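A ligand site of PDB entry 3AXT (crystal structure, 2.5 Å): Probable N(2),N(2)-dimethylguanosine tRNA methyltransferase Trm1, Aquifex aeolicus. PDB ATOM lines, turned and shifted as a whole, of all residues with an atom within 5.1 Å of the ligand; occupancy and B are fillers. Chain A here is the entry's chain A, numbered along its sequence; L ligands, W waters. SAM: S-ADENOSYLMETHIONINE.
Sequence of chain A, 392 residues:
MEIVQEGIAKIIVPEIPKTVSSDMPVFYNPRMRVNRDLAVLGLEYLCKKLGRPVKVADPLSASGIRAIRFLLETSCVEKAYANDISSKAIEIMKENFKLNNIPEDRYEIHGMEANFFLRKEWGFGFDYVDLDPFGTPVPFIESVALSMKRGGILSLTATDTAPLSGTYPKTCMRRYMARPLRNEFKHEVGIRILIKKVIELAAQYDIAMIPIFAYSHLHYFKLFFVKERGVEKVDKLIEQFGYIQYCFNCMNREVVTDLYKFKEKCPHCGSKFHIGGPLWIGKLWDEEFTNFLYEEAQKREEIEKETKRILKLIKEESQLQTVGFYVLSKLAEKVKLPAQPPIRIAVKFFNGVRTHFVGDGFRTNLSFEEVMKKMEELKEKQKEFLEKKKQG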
ATOM      1  N   PHE A  27      18.996 -19.236 -12.932  1.00  0.00           N
ATOM      2  CA  PHE A  27      17.594 -18.983 -13.250  1.00  0.00           C
ATOM      3  C   PHE A  27      16.838 -20.288 -13.535  1.00  0.00           C
ATOM      4  O   PHE A  27      15.747 -20.500 -13.002  1.00  0.00           O
ATOM      5  CB  PHE A  27      17.475 -18.030 -14.439  1.00  0.00           C
ATOM      6  CG  PHE A  27      16.091 -17.496 -14.645  1.00  0.00           C
ATOM      7  CD1 PHE A  27      15.366 -17.835 -15.772  1.00  0.00           C
ATOM      8  CD2 PHE A  27      15.511 -16.663 -13.706  1.00  0.00           C
ATOM      9  CE1 PHE A  27      14.091 -17.341 -15.961  1.00  0.00           C
ATOM     10  CE2 PHE A  27      14.243 -16.162 -13.891  1.00  0.00           C
ATOM     11  CZ  PHE A  27      13.525 -16.504 -15.025  1.00  0.00           C
ATOM     12  N   TYR A  28      17.437 -21.145 -14.349  1.00  0.00           N
ATOM     13  CA  TYR A  28      16.858 -22.456 -14.637  1.00  0.00           C
ATOM     14  C   TYR A  28      17.931 -23.533 -14.607  1.00  0.00           C
ATOM     15  O   TYR A  28      18.939 -23.437 -15.301  1.00  0.00           O
ATOM     16  CB  TYR A  28      16.159 -22.456 -16.003  1.00  0.00           C
ATOM     17  CG  TYR A  28      15.805 -23.847 -16.492  1.00  0.00           C
ATOM     18  CD1 TYR A  28      16.625 -24.514 -17.394  1.00  0.00           C
ATOM     19  CD2 TYR A  28      14.661 -24.488 -16.036  1.00  0.00           C
ATOM     20  CE1 TYR A  28      16.302 -25.779 -17.842  1.00  0.00           C
ATOM     21  CE2 TYR A  28      14.336 -25.766 -16.481  1.00  0.00           C
ATOM     22  CZ  TYR A  28      15.161 -26.396 -17.379  1.00  0.00           C
ATOM     23  OH  TYR A  28      14.838 -27.661 -17.827  1.00  0.00           O
ATOM     24  N   ARG A  36      11.160 -31.502 -10.452  1.00  0.00           N
ATOM     25  CA  ARG A  36       9.943 -30.973 -11.066  1.00  0.00           C
ATOM     26  C   ARG A  36       9.010 -32.071 -11.561  1.00  0.00           C
ATOM     27  O   ARG A  36       7.790 -31.904 -11.567  1.00  0.00           O
ATOM     28  CB  ARG A  36      10.292 -29.996 -12.196  1.00  0.00           C
ATOM     29  CG  ARG A  36      10.812 -28.646 -11.709  1.00  0.00           C
ATOM     30  CD  ARG A  36      11.090 -27.700 -12.879  1.00  0.00           C
ATOM     31  NE  ARG A  36      12.223 -28.130 -13.677  1.00  0.00           N
ATOM     32  CZ  ARG A  36      13.469 -27.719 -13.490  1.00  0.00           C
ATOM     33  NH1 ARG A  36      14.446 -28.174 -14.267  1.00  0.00           N
ATOM     34  NH2 ARG A  36      13.740 -26.861 -12.519  1.00  0.00           N
ATOM     35  N   ASP A  58       2.945 -21.014  -6.977  1.00  0.00           N
ATOM     36  CA  ASP A  58       4.375 -21.098  -7.257  1.00  0.00           C
ATOM     37  C   ASP A  58       5.052 -19.816  -6.784  1.00  0.00           C
ATOM     38  O   ASP A  58       5.396 -18.963  -7.591  1.00  0.00           O
ATOM     39  CB  ASP A  58       4.614 -21.309  -8.751  1.00  0.00           C
ATOM     40  CG  ASP A  58       6.055 -21.660  -9.080  1.00  0.00           C
ATOM     41  OD1 ASP A  58       6.931 -21.498  -8.200  1.00  0.00           O
ATOM     42  OD2 ASP A  58       6.314 -22.109 -10.215  1.00  0.00           O
ATOM     43  N   PRO A  59       5.235 -19.681  -5.464  1.00  0.00           N
ATOM     44  CA  PRO A  59       5.739 -18.459  -4.819  1.00  0.00           C
ATOM     45  C   PRO A  59       7.140 -18.049  -5.305  1.00  0.00           C
ATOM     46  O   PRO A  59       7.437 -16.864  -5.360  1.00  0.00           O
ATOM     47  CB  PRO A  59       5.785 -18.830  -3.331  1.00  0.00           C
ATOM     48  CG  PRO A  59       5.845 -20.323  -3.313  1.00  0.00           C
ATOM     49  CD  PRO A  59       5.023 -20.755  -4.483  1.00  0.00           C
ATOM     50  N   LEU A  60       7.974 -19.036  -5.628  1.00  0.00           N
ATOM     51  CA  LEU A  60       9.303 -18.764  -6.145  1.00  0.00           C
ATOM     52  C   LEU A  60       9.422 -19.393  -7.529  1.00  0.00           C
ATOM     53  O   LEU A  60       9.965 -20.485  -7.688  1.00  0.00           O
ATOM     54  CB  LEU A  60      10.369 -19.345  -5.216  1.00  0.00           C
ATOM     55  CG  LEU A  60      10.238 -18.961  -3.741  1.00  0.00           C
ATOM     56  CD1 LEU A  60      11.242 -19.707  -2.894  1.00  0.00           C
ATOM     57  CD2 LEU A  60      10.387 -17.458  -3.569  1.00  0.00           C
ATOM     58  N   SER A  61       8.909 -18.681  -8.529  1.00  0.00           N
ATOM     59  CA  SER A  61       8.666 -19.251  -9.846  1.00  0.00           C
ATOM     60  C   SER A  61       9.865 -19.193 -10.787  1.00  0.00           C
ATOM     61  O   SER A  61      10.090 -20.126 -11.567  1.00  0.00           O
ATOM     62  CB  SER A  61       7.464 -18.554 -10.492  1.00  0.00           C
ATOM     63  OG  SER A  61       7.035 -19.249 -11.654  1.00  0.00           O
ATOM     64  N   ALA A  62      10.638 -18.120 -10.713  1.00  0.00           N
ATOM     65  CA  ALA A  62      11.782 -17.917 -11.602  1.00  0.00           C
ATOM     66  C   ALA A  62      11.348 -17.870 -13.064  1.00  0.00           C
ATOM     67  O   ALA A  62      10.815 -16.858 -13.529  1.00  0.00           O
ATOM     68  CB  ALA A  62      12.821 -18.999 -11.390  1.00  0.00           C
ATOM     69  N   SER A  63      11.583 -18.956 -13.794  1.00  0.00           N
ATOM     70  CA  SER A  63      11.210 -19.027 -15.200  1.00  0.00           C
ATOM     71  C   SER A  63       9.723 -19.327 -15.354  1.00  0.00           C
ATOM     72  O   SER A  63       9.147 -19.098 -16.422  1.00  0.00           O
ATOM     73  CB  SER A  63      12.038 -20.094 -15.922  1.00  0.00           C
ATOM     74  OG  SER A  63      11.658 -21.396 -15.522  1.00  0.00           O
ATOM     75  N   ILE A  65       8.565 -22.373 -14.903  1.00  0.00           N
ATOM     76  CA  ILE A  65       8.504 -23.719 -15.445  1.00  0.00           C
ATOM     77  C   ILE A  65       7.547 -24.649 -14.698  1.00  0.00           C
ATOM     78  O   ILE A  65       6.790 -25.393 -15.313  1.00  0.00           O
ATOM     79  CB  ILE A  65       9.908 -24.362 -15.492  1.00  0.00           C
ATOM     80  CG1 ILE A  65       9.827 -25.794 -16.036  1.00  0.00           C
ATOM     81  CG2 ILE A  65      10.562 -24.337 -14.119  1.00  0.00           C
ATOM     82  CD1 ILE A  65       9.279 -25.889 -17.440  1.00  0.00           C
ATOM     83  N   ARG A  66       7.573 -24.592 -13.368  1.00  0.00           N
ATOM     84  CA  ARG A  66       6.729 -25.468 -12.565  1.00  0.00           C
ATOM     85  C   ARG A  66       5.244 -25.192 -12.771  1.00  0.00           C
ATOM     86  O   ARG A  66       4.467 -26.111 -13.046  1.00  0.00           O
ATOM     87  CB  ARG A  66       7.079 -25.357 -11.082  1.00  0.00           C
ATOM     88  CG  ARG A  66       8.443 -25.930 -10.711  1.00  0.00           C
ATOM     89  CD  ARG A  66       8.689 -25.871  -9.221  1.00  0.00           C
ATOM     90  NE  ARG A  66      10.048 -26.270  -8.862  1.00  0.00           N
ATOM     91  CZ  ARG A  66      10.386 -27.464  -8.399  1.00  0.00           C
ATOM     92  NH1 ARG A  66      11.646 -27.723  -8.097  1.00  0.00           N
ATOM     93  NH2 ARG A  66       9.460 -28.394  -8.215  1.00  0.00           N
ATOM     94  N   ASN A  83       4.699 -16.453  -8.792  1.00  0.00           N
ATOM     95  CA  ASN A  83       5.241 -15.224  -8.228  1.00  0.00           C
ATOM     96  C   ASN A  83       6.766 -15.231  -8.152  1.00  0.00           C
ATOM     97  O   ASN A  83       7.387 -16.271  -7.990  1.00  0.00           O
ATOM     98  CB  ASN A  83       4.646 -14.971  -6.839  1.00  0.00           C
ATOM     99  CG  ASN A  83       5.300 -13.814  -6.116  1.00  0.00           C
ATOM    100  OD1 ASN A  83       4.890 -12.658  -6.265  1.00  0.00           O
ATOM    101  ND2 ASN A  83       6.327 -14.107  -5.326  1.00  0.00           N
ATOM    102  N   ASP A  84       7.357 -14.042  -8.273  1.00  0.00           N
ATOM    103  CA  ASP A  84       8.796 -13.867  -8.132  1.00  0.00           C
ATOM    104  C   ASP A  84       9.121 -12.394  -7.941  1.00  0.00           C
ATOM    105  O   ASP A  84       8.600 -11.533  -8.650  1.00  0.00           O
ATOM    106  CB  ASP A  84       9.530 -14.416  -9.355  1.00  0.00           C
ATOM    107  CG  ASP A  84      10.993 -14.716  -9.062  1.00  0.00           C
ATOM    108  OD1 ASP A  84      11.778 -13.757  -8.879  1.00  0.00           O
ATOM    109  OD2 ASP A  84      11.360 -15.915  -9.036  1.00  0.00           O
ATOM    110  N   ILE A  85      10.006 -12.103  -6.987  1.00  0.00           N
ATOM    111  CA  ILE A  85      10.342 -10.725  -6.666  1.00  0.00           C
ATOM    112  C   ILE A  85      11.271 -10.110  -7.720  1.00  0.00           C
ATOM    113  O   ILE A  85      11.453  -8.894  -7.765  1.00  0.00           O
ATOM    114  CB  ILE A  85      11.026 -10.625  -5.292  1.00  0.00           C
ATOM    115  CG1 ILE A  85      10.921  -9.200  -4.735  1.00  0.00           C
ATOM    116  CG2 ILE A  85      12.477 -11.087  -5.375  1.00  0.00           C
ATOM    117  CD1 ILE A  85      11.464  -9.059  -3.324  1.00  0.00           C
ATOM    118  N   SER A  86      11.830 -10.952  -8.576  1.00  0.00           N
ATOM    119  CA  SER A  86      12.754 -10.492  -9.607  1.00  0.00           C
ATOM    120  C   SER A  86      12.006  -9.983 -10.837  1.00  0.00           C
ATOM    121  O   SER A  86      11.048 -10.596 -11.305  1.00  0.00           O
ATOM    122  CB  SER A  86      13.728 -11.602 -10.010  1.00  0.00           C
ATOM    123  OG  SER A  86      14.548 -11.197 -11.088  1.00  0.00           O
ATOM    124  N   MET A 112       5.811  -9.997  -6.035  1.00  0.00           N
ATOM    125  CA  MET A 112       5.865  -9.667  -4.624  1.00  0.00           C
ATOM    126  C   MET A 112       6.864 -10.561  -3.911  1.00  0.00           C
ATOM    127  O   MET A 112       7.321 -11.561  -4.452  1.00  0.00           O
ATOM    128  CB  MET A 112       4.487  -9.836  -3.992  1.00  0.00           C
ATOM    129  CG  MET A 112       3.368  -9.085  -4.694  1.00  0.00           C
ATOM    130  SD  MET A 112       1.737  -9.607  -4.140  1.00  0.00           S
ATOM    131  CE  MET A 112       1.871  -9.321  -2.370  1.00  0.00           C
ATOM    132  N   GLU A 113       7.200 -10.186  -2.677  1.00  0.00           N
ATOM    133  CA  GLU A 113       7.983 -11.049  -1.823  1.00  0.00           C
ATOM    134  C   GLU A 113       7.133 -12.262  -1.467  1.00  0.00           C
ATOM    135  O   GLU A 113       5.956 -12.118  -1.115  1.00  0.00           O
ATOM    136  CB  GLU A 113       8.429 -10.303  -0.566  1.00  0.00           C
ATOM    137  CG  GLU A 113       9.551 -10.975   0.209  1.00  0.00           C
ATOM    138  CD  GLU A 113       9.051 -12.092   1.094  1.00  0.00           C
ATOM    139  OE1 GLU A 113       7.863 -12.057   1.476  1.00  0.00           O
ATOM    140  OE2 GLU A 113       9.842 -13.005   1.409  1.00  0.00           O
ATOM    141  N   ALA A 114       7.717 -13.454  -1.567  1.00  0.00           N
ATOM    142  CA  ALA A 114       6.993 -14.709  -1.389  1.00  0.00           C
ATOM    143  C   ALA A 114       5.977 -14.692  -0.248  1.00  0.00           C
ATOM    144  O   ALA A 114       4.824 -15.085  -0.441  1.00  0.00           O
ATOM    145  CB  ALA A 114       7.978 -15.858  -1.203  1.00  0.00           C
ATOM    146  N   ASP A 132      10.288 -23.830  -3.866  1.00  0.00           N
ATOM    147  CA  ASP A 132      11.599 -24.220  -4.387  1.00  0.00           C
ATOM    148  C   ASP A 132      12.600 -23.069  -4.285  1.00  0.00           C
ATOM    149  O   ASP A 132      12.835 -22.350  -5.258  1.00  0.00           O
ATOM    150  CB  ASP A 132      11.466 -24.675  -5.840  1.00  0.00           C
ATOM    151  CG  ASP A 132      12.803 -25.068  -6.462  1.00  0.00           C
ATOM    152  OD1 ASP A 132      13.663 -25.602  -5.726  1.00  0.00           O
ATOM    153  OD2 ASP A 132      12.984 -24.836  -7.676  1.00  0.00           O
ATOM    154  N   PRO A 133      13.201 -22.884  -3.090  1.00  0.00           N
ATOM    155  CA  PRO A 133      14.129 -21.786  -2.839  1.00  0.00           C
ATOM    156  C   PRO A 133      15.603 -22.186  -2.965  1.00  0.00           C
ATOM    157  O   PRO A 133      15.934 -23.375  -2.919  1.00  0.00           O
ATOM    158  CB  PRO A 133      13.840 -21.447  -1.382  1.00  0.00           C
ATOM    159  CG  PRO A 133      13.535 -22.784  -0.772  1.00  0.00           C
ATOM    160  CD  PRO A 133      12.854 -23.606  -1.853  1.00  0.00           C
ATOM    161  N   PHE A 134      16.465 -21.190  -3.132  1.00  0.00           N
ATOM    162  CA  PHE A 134      17.905 -21.410  -3.031  1.00  0.00           C
ATOM    163  C   PHE A 134      18.278 -21.451  -1.556  1.00  0.00           C
ATOM    164  O   PHE A 134      18.216 -20.435  -0.867  1.00  0.00           O
ATOM    165  CB  PHE A 134      18.678 -20.279  -3.711  1.00  0.00           C
ATOM    166  CG  PHE A 134      18.586 -20.274  -5.208  1.00  0.00           C
ATOM    167  CD1 PHE A 134      18.771 -21.446  -5.939  1.00  0.00           C
ATOM    168  CD2 PHE A 134      18.319 -19.105  -5.893  1.00  0.00           C
ATOM    169  CE1 PHE A 134      18.685 -21.435  -7.319  1.00  0.00           C
ATOM    170  CE2 PHE A 134      18.233 -19.094  -7.273  1.00  0.00           C
ATOM    171  CZ  PHE A 134      18.418 -20.257  -7.993  1.00  0.00           C
ATOM    172  N   PHE A 140       9.800 -19.399   4.585  1.00  0.00           N
ATOM    173  CA  PHE A 140       8.528 -19.403   3.875  1.00  0.00           C
ATOM    174  C   PHE A 140       7.528 -20.403   4.438  1.00  0.00           C
ATOM    175  O   PHE A 140       6.350 -20.384   4.073  1.00  0.00           O
ATOM    176  CB  PHE A 140       8.747 -19.689   2.390  1.00  0.00           C
ATOM    177  CG  PHE A 140       9.865 -18.891   1.769  1.00  0.00           C
ATOM    178  CD1 PHE A 140      11.104 -19.467   1.559  1.00  0.00           C
ATOM    179  CD2 PHE A 140       9.675 -17.567   1.410  1.00  0.00           C
ATOM    180  CE1 PHE A 140      12.137 -18.737   0.997  1.00  0.00           C
ATOM    181  CE2 PHE A 140      10.697 -16.837   0.838  1.00  0.00           C
ATOM    182  CZ  PHE A 140      11.927 -17.424   0.638  1.00  0.00           C
HETATM  183  N   SAM L   1      11.004 -22.661  -8.971  1.00  0.00           N
HETATM  184  CA  SAM L   1      11.907 -22.486 -10.101  1.00  0.00           C
HETATM  185  C   SAM L   1      12.310 -23.820 -10.726  1.00  0.00           C
HETATM  186  O   SAM L   1      13.065 -23.866 -11.702  1.00  0.00           O
HETATM  187  OXT SAM L   1      11.890 -24.886 -10.278  1.00  0.00           O
HETATM  188  CB  SAM L   1      13.131 -21.680  -9.696  1.00  0.00           C
HETATM  189  CG  SAM L   1      13.228 -21.374  -8.208  1.00  0.00           C
HETATM  190  SD  SAM L   1      14.677 -20.365  -7.780  1.00  0.00           S
HETATM  191  CE  SAM L   1      15.509 -21.528  -6.674  1.00  0.00           C
HETATM  192  C5' SAM L   1      14.004 -19.201  -6.569  1.00  0.00           C
HETATM  193  C4' SAM L   1      13.549 -17.869  -7.162  1.00  0.00           C
HETATM  194  O4' SAM L   1      12.797 -17.178  -6.176  1.00  0.00           O
HETATM  195  C3' SAM L   1      14.688 -16.955  -7.565  1.00  0.00           C
HETATM  196  O3' SAM L   1      14.656 -16.737  -8.957  1.00  0.00           O
HETATM  197  C2' SAM L   1      14.456 -15.643  -6.844  1.00  0.00           C
HETATM  198  O2' SAM L   1      14.433 -14.562  -7.750  1.00  0.00           O
HETATM  199  C1' SAM L   1      13.092 -15.789  -6.194  1.00  0.00           C
HETATM  200  N9  SAM L   1      13.113 -15.290  -4.817  1.00  0.00           N
HETATM  201  C8  SAM L   1      14.158 -15.385  -3.928  1.00  0.00           C
HETATM  202  N7  SAM L   1      13.774 -14.813  -2.769  1.00  0.00           N
HETATM  203  C5  SAM L   1      12.511 -14.366  -2.888  1.00  0.00           C
HETATM  204  C6  SAM L   1      11.657 -13.712  -2.012  1.00  0.00           C
HETATM  205  N6  SAM L   1      12.064 -13.417  -0.783  1.00  0.00           N
HETATM  206  N1  SAM L   1      10.389 -13.355  -2.428  1.00  0.00           N
HETATM  207  C2  SAM L   1       9.981 -13.667  -3.708  1.00  0.00           C
HETATM  208  N3  SAM L   1      10.828 -14.319  -4.577  1.00  0.00           N
HETATM  209  C4  SAM L   1      12.072 -14.659  -4.176  1.00  0.00           C
HETATM  210  O   HOH W   1      13.299 -21.773 -13.442  1.00  0.00           O
HETATM  211  O   HOH W   2       8.725 -22.607 -11.524  1.00  0.00           O
HETATM  212  O   HOH W   3      15.680 -24.530 -11.833  1.00  0.00           O
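The guanidinium group of Arg 66 is in salt-bridge range of an oxygen (OXT) of the ligand (2.7 Å).
A nitrogen (N) of the ligand lies within hydrogen-bond range of the backbone carbonyl oxygen (O) of Leu 60 (2.7 Å).
A nitrogen (N1) of the ligand lies within hydrogen-bond range of the backbone NH (N) of Ala 114, 2.8 Å away.
OD2 of Asp 132 is in salt-bridge range of N of the ligand (3.2 Å).
An oxygen (O2') of the ligand is in hydrogen-bond range of the side-chain carboxylate (OD1) of Asp 84, at 3.0 Å.
The side-chain carboxylate (OE2) of Glu 113 sits at hydrogen-bond distance from a nitrogen (N6) of the ligand (3.1 Å).
The guanidinium group (NH2) of Arg 36 lies within salt-bridge range of an oxygen (O) of the ligand (3.2 Å).
The backbone NH (N) of Ile 85 lies within hydrogen-bond range of a nitrogen (N3) of the ligand.
OD2 of Asp 132 lies within salt-bridge range of NH1 of Arg 66 (3.2 Å).
OD2 of Asp 84 sits at hydrogen-bond distance from N of Ala 62 (2.9 Å).
N of Ser 86 sits at hydrogen-bond distance from OD1 of Asp 84 (2.8 Å).
The backbone NH of Ser 61 sits at hydrogen-bond distance from the backbone carbonyl oxygen of Asn 83.
The side-chain hydroxyl (OG) of Ser 61 is in hydrogen-bond range of the side-chain carboxylate (OD2) of Asp 58 (3.3 Å).
The backbone NH (N) of Met 112 sits at hydrogen-bond distance from the side-chain amide oxygen (OD1) of Asn 83 (2.8 Å).
N of Ile 65 lies close to OG of Ser 63, at 3.3 Å.
Residues that only touch the ligand: Ser 61, Ala 62, Ile 65, Ser 86, Met 112, Pro 133 and Phe 134.
Water W3 bridges an oxygen (O) of the ligand (2.7 Å) and the guanidinium group of Arg 36 (3.1 Å).
Water W1 lies within hydrogen-bond range of OG of Ser 63 (2.7 Å), O of the ligand (2.7 Å) and O of Phe 27 (2.8 Å).
Water W2 lies within hydrogen-bond range of the side-chain carboxylate (OD2) of Asp 58, the backbone carbonyl oxygen (O) of Ser 61, the backbone NH (N) of Arg 66, the backbone NH (N) of Ile 65 and a nitrogen (N) of the ligand.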
